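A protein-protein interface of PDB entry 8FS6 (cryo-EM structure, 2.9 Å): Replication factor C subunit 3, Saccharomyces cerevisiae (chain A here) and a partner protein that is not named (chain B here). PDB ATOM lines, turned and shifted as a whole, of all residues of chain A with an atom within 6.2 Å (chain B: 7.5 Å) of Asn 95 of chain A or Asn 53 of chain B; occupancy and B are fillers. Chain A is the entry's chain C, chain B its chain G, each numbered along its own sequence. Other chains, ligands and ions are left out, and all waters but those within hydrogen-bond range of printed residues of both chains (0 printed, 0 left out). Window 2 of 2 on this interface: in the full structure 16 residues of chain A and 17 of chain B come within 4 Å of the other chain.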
ATOM      1  N   LEU A  80     -19.019  26.381  27.959  1.00  0.00           N
ATOM      2  CA  LEU A  80     -18.429  25.088  28.294  1.00  0.00           C
ATOM      3  C   LEU A  80     -17.476  25.322  29.464  1.00  0.00           C
ATOM      4  O   LEU A  80     -16.303  25.648  29.275  1.00  0.00           O
ATOM      5  CB  LEU A  80     -17.713  24.475  27.093  1.00  0.00           C
ATOM      6  CG  LEU A  80     -17.074  23.102  27.312  1.00  0.00           C
ATOM      7  CD1 LEU A  80     -18.140  22.044  27.543  1.00  0.00           C
ATOM      8  CD2 LEU A  80     -16.188  22.729  26.134  1.00  0.00           C
ATOM      9  N   ILE A  90      -5.220  15.758  27.445  1.00  0.00           N
ATOM     10  CA  ILE A  90      -5.058  16.037  26.023  1.00  0.00           C
ATOM     11  C   ILE A  90      -6.182  15.413  25.202  1.00  0.00           C
ATOM     12  O   ILE A  90      -6.620  16.006  24.207  1.00  0.00           O
ATOM     13  CB  ILE A  90      -3.663  15.580  25.541  1.00  0.00           C
ATOM     14  CG1 ILE A  90      -3.357  16.145  24.151  1.00  0.00           C
ATOM     15  CG2 ILE A  90      -3.520  14.060  25.572  1.00  0.00           C
ATOM     16  CD1 ILE A  90      -2.029  15.689  23.585  1.00  0.00           C
ATOM     17  N   ASP A  91      -6.675  14.237  25.604  1.00  0.00           N
ATOM     18  CA  ASP A  91      -7.794  13.620  24.900  1.00  0.00           C
ATOM     19  C   ASP A  91      -9.052  14.470  25.010  1.00  0.00           C
ATOM     20  O   ASP A  91      -9.773  14.646  24.025  1.00  0.00           O
ATOM     21  CB  ASP A  91      -8.048  12.215  25.444  1.00  0.00           C
ATOM     22  CG  ASP A  91      -6.767  11.456  25.718  1.00  0.00           C
ATOM     23  OD1 ASP A  91      -5.948  11.938  26.528  1.00  0.00           O
ATOM     24  OD2 ASP A  91      -6.576  10.376  25.120  1.00  0.00           O
ATOM     25  N   VAL A  92      -9.328  15.012  26.198  1.00  0.00           N
ATOM     26  CA  VAL A  92     -10.483  15.889  26.354  1.00  0.00           C
ATOM     27  C   VAL A  92     -10.287  17.182  25.572  1.00  0.00           C
ATOM     28  O   VAL A  92     -11.213  17.659  24.906  1.00  0.00           O
ATOM     29  CB  VAL A  92     -10.763  16.143  27.845  1.00  0.00           C
ATOM     30  CG1 VAL A  92     -11.654  17.358  28.028  1.00  0.00           C
ATOM     31  CG2 VAL A  92     -11.449  14.925  28.430  1.00  0.00           C
ATOM     32  N   VAL A  93      -9.074  17.741  25.598  1.00  0.00           N
ATOM     33  CA  VAL A  93      -8.786  18.953  24.835  1.00  0.00           C
ATOM     34  C   VAL A  93      -9.040  18.730  23.348  1.00  0.00           C
ATOM     35  O   VAL A  93      -9.565  19.614  22.660  1.00  0.00           O
ATOM     36  CB  VAL A  93      -7.338  19.413  25.109  1.00  0.00           C
ATOM     37  CG1 VAL A  93      -6.827  20.323  24.000  1.00  0.00           C
ATOM     38  CG2 VAL A  93      -7.255  20.118  26.454  1.00  0.00           C
ATOM     39  N   ARG A  94      -8.707  17.546  22.837  1.00  0.00           N
ATOM     40  CA  ARG A  94      -8.883  17.256  21.421  1.00  0.00           C
ATOM     41  C   ARG A  94     -10.261  16.708  21.059  1.00  0.00           C
ATOM     42  O   ARG A  94     -10.603  16.690  19.872  1.00  0.00           O
ATOM     43  CB  ARG A  94      -7.815  16.259  20.956  1.00  0.00           C
ATOM     44  CG  ARG A  94      -6.418  16.851  20.868  1.00  0.00           C
ATOM     45  CD  ARG A  94      -5.410  15.826  20.382  1.00  0.00           C
ATOM     46  NE  ARG A  94      -5.646  14.507  20.956  1.00  0.00           N
ATOM     47  CZ  ARG A  94      -4.717  13.570  21.083  1.00  0.00           C
ATOM     48  NH1 ARG A  94      -3.471  13.773  20.688  1.00  0.00           N
ATOM     49  NH2 ARG A  94      -5.047  12.398  21.620  1.00  0.00           N
ATOM     50  N   ASN A  95     -11.059  16.268  22.033  1.00  0.00           N
ATOM     51  CA  ASN A  95     -12.304  15.563  21.745  1.00  0.00           C
ATOM     52  C   ASN A  95     -13.558  16.249  22.269  1.00  0.00           C
ATOM     53  O   ASN A  95     -14.664  15.836  21.915  1.00  0.00           O
ATOM     54  CB  ASN A  95     -12.246  14.145  22.323  1.00  0.00           C
ATOM     55  CG  ASN A  95     -11.320  13.236  21.544  1.00  0.00           C
ATOM     56  OD1 ASN A  95     -10.735  13.638  20.538  1.00  0.00           O
ATOM     57  ND2 ASN A  95     -11.176  12.001  22.010  1.00  0.00           N
ATOM     58  N   GLN A  96     -13.439  17.246  23.142  1.00  0.00           N
ATOM     59  CA  GLN A  96     -14.597  18.001  23.603  1.00  0.00           C
ATOM     60  C   GLN A  96     -14.462  19.489  23.311  1.00  0.00           C
ATOM     61  O   GLN A  96     -15.358  20.089  22.708  1.00  0.00           O
ATOM     62  CB  GLN A  96     -14.811  17.778  25.105  1.00  0.00           C
ATOM     63  CG  GLN A  96     -16.014  18.515  25.676  1.00  0.00           C
ATOM     64  CD  GLN A  96     -16.316  18.121  27.110  1.00  0.00           C
ATOM     65  OE1 GLN A  96     -15.490  17.509  27.785  1.00  0.00           O
ATOM     66  NE2 GLN A  96     -17.506  18.476  27.582  1.00  0.00           N
ATOM     67  N   ILE A  97     -13.343  20.088  23.722  1.00  0.00           N
ATOM     68  CA  ILE A  97     -13.114  21.511  23.494  1.00  0.00           C
ATOM     69  C   ILE A  97     -13.044  21.809  22.002  1.00  0.00           C
ATOM     70  O   ILE A  97     -13.614  22.797  21.523  1.00  0.00           O
ATOM     71  CB  ILE A  97     -11.833  21.962  24.222  1.00  0.00           C
ATOM     72  CG1 ILE A  97     -11.899  21.586  25.703  1.00  0.00           C
ATOM     73  CG2 ILE A  97     -11.622  23.455  24.056  1.00  0.00           C
ATOM     74  CD1 ILE A  97     -10.684  22.016  26.497  1.00  0.00           C
ATOM     75  N   LYS A  98     -12.345  20.958  21.246  1.00  0.00           N
ATOM     76  CA  LYS A  98     -12.176  21.190  19.817  1.00  0.00           C
ATOM     77  C   LYS A  98     -13.492  21.140  19.052  1.00  0.00           C
ATOM     78  O   LYS A  98     -13.712  21.984  18.179  1.00  0.00           O
ATOM     79  CB  LYS A  98     -11.196  20.174  19.229  1.00  0.00           C
ATOM     80  CG  LYS A  98     -10.694  20.539  17.842  1.00  0.00           C
ATOM     81  CD  LYS A  98     -10.037  19.353  17.157  1.00  0.00           C
ATOM     82  CE  LYS A  98      -8.720  19.752  16.515  1.00  0.00           C
ATOM     83  NZ  LYS A  98      -8.888  20.884  15.562  1.00  0.00           N
ATOM     84  N   ASP A  99     -14.373  20.187  19.354  1.00  0.00           N
ATOM     85  CA  ASP A  99     -15.658  20.127  18.671  1.00  0.00           C
ATOM     86  C   ASP A  99     -16.708  21.054  19.267  1.00  0.00           C
ATOM     87  O   ASP A  99     -17.732  21.297  18.620  1.00  0.00           O
ATOM     88  CB  ASP A  99     -16.192  18.692  18.645  1.00  0.00           C
ATOM     89  CG  ASP A  99     -15.088  17.666  18.528  1.00  0.00           C
ATOM     90  OD1 ASP A  99     -14.431  17.615  17.473  1.00  0.00           O
ATOM     91  OD2 ASP A  99     -14.878  16.905  19.494  1.00  0.00           O
ATOM     92  N   PHE A 100     -16.491  21.576  20.477  1.00  0.00           N
ATOM     93  CA  PHE A 100     -17.331  22.677  20.933  1.00  0.00           C
ATOM     94  C   PHE A 100     -16.953  23.975  20.235  1.00  0.00           C
ATOM     95  O   PHE A 100     -17.826  24.799  19.941  1.00  0.00           O
ATOM     96  CB  PHE A 100     -17.231  22.838  22.451  1.00  0.00           C
ATOM     97  CG  PHE A 100     -18.166  23.874  23.013  1.00  0.00           C
ATOM     98  CD1 PHE A 100     -19.495  23.567  23.254  1.00  0.00           C
ATOM     99  CD2 PHE A 100     -17.716  25.152  23.299  1.00  0.00           C
ATOM    100  CE1 PHE A 100     -20.357  24.519  23.770  1.00  0.00           C
ATOM    101  CE2 PHE A 100     -18.572  26.106  23.815  1.00  0.00           C
ATOM    102  CZ  PHE A 100     -19.894  25.789  24.051  1.00  0.00           C
ATOM    103  N   THR A 103     -18.041  23.570  16.065  1.00  0.00           N
ATOM    104  CA  THR A 103     -19.440  23.651  15.667  1.00  0.00           C
ATOM    105  C   THR A 103     -19.931  25.094  15.676  1.00  0.00           C
ATOM    106  O   THR A 103     -19.437  25.940  16.427  1.00  0.00           O
ATOM    107  CB  THR A 103     -20.310  22.796  16.589  1.00  0.00           C
ATOM    108  OG1 THR A 103     -19.956  23.048  17.954  1.00  0.00           O
ATOM    109  CG2 THR A 103     -20.114  21.319  16.280  1.00  0.00           C
ATOM    110  N   ASP B  35     -22.305   7.354  30.924  1.00  0.00           N
ATOM    111  CA  ASP B  35     -22.615   8.737  31.362  1.00  0.00           C
ATOM    112  C   ASP B  35     -24.029   8.765  31.934  1.00  0.00           C
ATOM    113  O   ASP B  35     -24.458   7.721  32.442  1.00  0.00           O
ATOM    114  CB  ASP B  35     -22.454   9.731  30.212  1.00  0.00           C
ATOM    115  CG  ASP B  35     -22.126  11.147  30.657  1.00  0.00           C
ATOM    116  OD1 ASP B  35     -21.740  11.322  31.828  1.00  0.00           O
ATOM    117  OD2 ASP B  35     -22.274  12.065  29.830  1.00  0.00           O
ATOM    118  N   GLU B  51     -27.519  14.011  25.482  1.00  0.00           N
ATOM    119  CA  GLU B  51     -26.728  14.998  24.758  1.00  0.00           C
ATOM    120  C   GLU B  51     -25.247  14.755  25.004  1.00  0.00           C
ATOM    121  O   GLU B  51     -24.848  14.351  26.100  1.00  0.00           O
ATOM    122  CB  GLU B  51     -27.093  16.428  25.178  1.00  0.00           C
ATOM    123  CG  GLU B  51     -28.586  16.712  25.210  1.00  0.00           C
ATOM    124  CD  GLU B  51     -28.897  18.189  25.328  1.00  0.00           C
ATOM    125  OE1 GLU B  51     -27.959  19.006  25.215  1.00  0.00           O
ATOM    126  OE2 GLU B  51     -30.079  18.534  25.532  1.00  0.00           O
ATOM    127  N   ASN B  52     -24.432  15.010  23.979  1.00  0.00           N
ATOM    128  CA  ASN B  52     -22.984  14.847  24.059  1.00  0.00           C
ATOM    129  C   ASN B  52     -22.308  16.133  23.610  1.00  0.00           C
ATOM    130  O   ASN B  52     -22.490  16.562  22.465  1.00  0.00           O
ATOM    131  CB  ASN B  52     -22.509  13.671  23.200  1.00  0.00           C
ATOM    132  CG  ASN B  52     -22.741  12.330  23.863  1.00  0.00           C
ATOM    133  OD1 ASN B  52     -23.307  12.250  24.954  1.00  0.00           O
ATOM    134  ND2 ASN B  52     -22.299  11.263  23.208  1.00  0.00           N
ATOM    135  N   ASN B  53     -21.537  16.743  24.512  1.00  0.00           N
ATOM    136  CA  ASN B  53     -20.674  17.889  24.223  1.00  0.00           C
ATOM    137  C   ASN B  53     -21.437  19.093  23.675  1.00  0.00           C
ATOM    138  O   ASN B  53     -20.844  19.949  23.012  1.00  0.00           O
ATOM    139  CB  ASN B  53     -19.548  17.504  23.255  1.00  0.00           C
ATOM    140  CG  ASN B  53     -18.612  16.462  23.834  1.00  0.00           C
ATOM    141  OD1 ASN B  53     -18.740  16.073  24.994  1.00  0.00           O
ATOM    142  ND2 ASN B  53     -17.664  16.005  23.025  1.00  0.00           N
ATOM    143  N   HIS B  54     -22.743  19.172  23.940  1.00  0.00           N
ATOM    144  CA  HIS B  54     -23.614  20.253  23.477  1.00  0.00           C
ATOM    145  C   HIS B  54     -23.610  20.407  21.958  1.00  0.00           C
ATOM    146  O   HIS B  54     -23.944  21.476  21.439  1.00  0.00           O
ATOM    147  CB  HIS B  54     -23.254  21.590  24.137  1.00  0.00           C
ATOM    148  CG  HIS B  54     -22.923  21.479  25.592  1.00  0.00           C
ATOM    149  ND1 HIS B  54     -21.646  21.237  26.049  1.00  0.00           N
ATOM    150  CD2 HIS B  54     -23.704  21.582  26.695  1.00  0.00           C
ATOM    151  CE1 HIS B  54     -21.653  21.193  27.370  1.00  0.00           C
ATOM    152  NE2 HIS B  54     -22.890  21.400  27.786  1.00  0.00           N
ATOM    153  N   VAL B  55     -23.237  19.358  21.227  1.00  0.00           N
ATOM    154  CA  VAL B  55     -23.208  19.407  19.772  1.00  0.00           C
ATOM    155  C   VAL B  55     -24.194  18.438  19.134  1.00  0.00           C
ATOM    156  O   VAL B  55     -24.505  18.594  17.943  1.00  0.00           O
ATOM    157  CB  VAL B  55     -21.787  19.153  19.230  1.00  0.00           C
ATOM    158  CG1 VAL B  55     -20.829  20.222  19.730  1.00  0.00           C
ATOM    159  CG2 VAL B  55     -21.304  17.766  19.626  1.00  0.00           C
ATOM    160  N   ILE B  56     -24.693  17.448  19.873  1.00  0.00           N
ATOM    161  CA  ILE B  56     -25.677  16.508  19.355  1.00  0.00           C
ATOM    162  C   ILE B  56     -26.584  16.088  20.503  1.00  0.00           C
ATOM    163  O   ILE B  56     -26.145  15.952  21.648  1.00  0.00           O
ATOM    164  CB  ILE B  56     -25.000  15.290  18.678  1.00  0.00           C
ATOM    165  CG1 ILE B  56     -26.049  14.375  18.041  1.00  0.00           C
ATOM    166  CG2 ILE B  56     -24.124  14.529  19.664  1.00  0.00           C
ATOM    167  CD1 ILE B  56     -25.474  13.195  17.323  1.00  0.00           C
ATOM    168  N   LEU B 145     -30.513  22.669  21.455  1.00  0.00           N
ATOM    169  CA  LEU B 145     -30.249  21.801  20.306  1.00  0.00           C
ATOM    170  C   LEU B 145     -31.571  21.432  19.633  1.00  0.00           C
ATOM    171  O   LEU B 145     -31.998  20.275  19.598  1.00  0.00           O
ATOM    172  CB  LEU B 145     -29.476  20.564  20.739  1.00  0.00           C
ATOM    173  CG  LEU B 145     -27.950  20.665  20.713  1.00  0.00           C
ATOM    174  CD1 LEU B 145     -27.335  19.735  21.744  1.00  0.00           C
ATOM    175  CD2 LEU B 145     -27.428  20.347  19.324  1.00  0.00           C
ATOM    176  N   ASP B 238     -19.374  16.844  11.303  1.00  0.00           N
ATOM    177  CA  ASP B 238     -18.398  15.867  11.761  1.00  0.00           C
ATOM    178  C   ASP B 238     -19.047  14.490  11.803  1.00  0.00           C
ATOM    179  O   ASP B 238     -20.139  14.324  12.355  1.00  0.00           O
ATOM    180  CB  ASP B 238     -17.865  16.252  13.139  1.00  0.00           C
ATOM    181  CG  ASP B 238     -16.688  15.398  13.570  1.00  0.00           C
ATOM    182  OD1 ASP B 238     -16.104  14.706  12.711  1.00  0.00           O
ATOM    183  OD2 ASP B 238     -16.347  15.418  14.771  1.00  0.00           O
ATOM    184  N   THR B 240     -18.231  11.986  13.492  1.00  0.00           N
ATOM    185  CA  THR B 240     -18.354  11.458  14.847  1.00  0.00           C
ATOM    186  C   THR B 240     -19.771  11.641  15.372  1.00  0.00           C
ATOM    187  O   THR B 240     -20.343  10.726  15.975  1.00  0.00           O
ATOM    188  CB  THR B 240     -17.345  12.139  15.772  1.00  0.00           C
ATOM    189  OG1 THR B 240     -16.027  12.010  15.224  1.00  0.00           O
ATOM    190  CG2 THR B 240     -17.376  11.507  17.156  1.00  0.00           C
ATOM    191  N   SER B 241     -20.360  12.816  15.138  1.00  0.00           N
ATOM    192  CA  SER B 241     -21.755  13.042  15.495  1.00  0.00           C
ATOM    193  C   SER B 241     -22.715  12.404  14.497  1.00  0.00           C
ATOM    194  O   SER B 241     -23.810  11.982  14.882  1.00  0.00           O
ATOM    195  CB  SER B 241     -22.031  14.542  15.604  1.00  0.00           C
ATOM    196  OG  SER B 241     -21.145  15.158  16.521  1.00  0.00           O
ATOM    197  N   LYS B 244     -23.811   8.667  15.069  1.00  0.00           N
ATOM    198  CA  LYS B 244     -24.710   8.335  16.166  1.00  0.00           C
ATOM    199  C   LYS B 244     -26.096   7.928  15.682  1.00  0.00           C
ATOM    200  O   LYS B 244     -26.843   7.298  16.438  1.00  0.00           O
ATOM    201  CB  LYS B 244     -24.829   9.519  17.127  1.00  0.00           C
ATOM    202  CG  LYS B 244     -23.504  10.169  17.489  1.00  0.00           C
ATOM    203  CD  LYS B 244     -22.616   9.232  18.277  1.00  0.00           C
ATOM    204  CE  LYS B 244     -21.459   9.976  18.921  1.00  0.00           C
ATOM    205  NZ  LYS B 244     -21.927  11.056  19.833  1.00  0.00           N
ATOM    206  N   LEU B 311     -25.430  19.618  15.206  1.00  0.00           N
ATOM    207  CA  LEU B 311     -24.908  20.927  14.839  1.00  0.00           C
ATOM    208  C   LEU B 311     -23.918  20.810  13.687  1.00  0.00           C
ATOM    209  O   LEU B 311     -23.155  19.842  13.603  1.00  0.00           O
ATOM    210  CB  LEU B 311     -24.228  21.603  16.033  1.00  0.00           C
ATOM    211  CG  LEU B 311     -25.138  22.185  17.115  1.00  0.00           C
ATOM    212  CD1 LEU B 311     -24.313  22.735  18.268  1.00  0.00           C
ATOM    213  CD2 LEU B 311     -26.041  23.263  16.537  1.00  0.00           C
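The backbone carbonyl oxygen (O) of Asn 95 of chain A lies within hydrogen-bond range of the side-chain amide nitrogen (ND2) of Asn 53 of chain B.
The side-chain carboxylate (OD2) of Asp 99 of chain A sits close to the backbone carbonyl oxygen (O) of Asn 95 of chain A, 2.7 Å away. O of Asp 99 of chain A lies within hydrogen-bond range of OG1 of Thr 103 of chain A, 2.9 Å away. The backbone carbonyl oxygen of Phe 100 of chain A is in hydrogen-bond range of the side-chain hydroxyl of Thr 103 of chain A, 3.4 Å away. N of Leu 311 of chain B lies within hydrogen-bond range of O of Val 55 of chain B (3.1 Å). OG1 of Thr 240 of chain B lies within hydrogen-bond range of OD2 of Asp 238 of chain B, at 3.5 Å.
Among the printed residues, merely in contact across the chains: Leu 80 of chain A with His 54 of chain B (3.6 Å), Gln 96 of chain A with Asn 53 of chain B (3.7 Å), Asp 99 of chain A with Val 55 of chain B (3.5 Å), Asp 99 of chain A with Asp 238 of chain B (3.97 Å), Phe 100 of chain A with Asn 53 of chain B (3.9 Å) and Thr 103 of chain A with Val 55 of chain B (3.5 Å).
Asn 95 of chain A touches one residue of chain B. Of the printed residues of chain B, Phe 100 of chain A touches Asn 53. Of the printed residues of chain B, Thr 103 of chain A touches Val 55. Asn 53 of chain B touches three residues of chain A. Printed residues of chain A within 4 Å of Asp 238 of chain B: Asp 99. Lys 244 of chain B touches none of the printed residues of chain A. The nearest residue of chain B that does not touch Asn 95 of chain A is Thr 240 of chain B (7.0 Å). The nearest printed residue of chain B that does not touch Leu 80 of chain A is Asn 53 of chain B (5.7 Å).
Of the 13 printed residues of chain A, 6 touch a printed residue of chain B. Hydrophobic or aromatic side chains of chain B that line the printed part of chain A: His 54 and Val 55. Along chain B the printed residues that touch a printed residue of chain A span positions 53 to 238.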
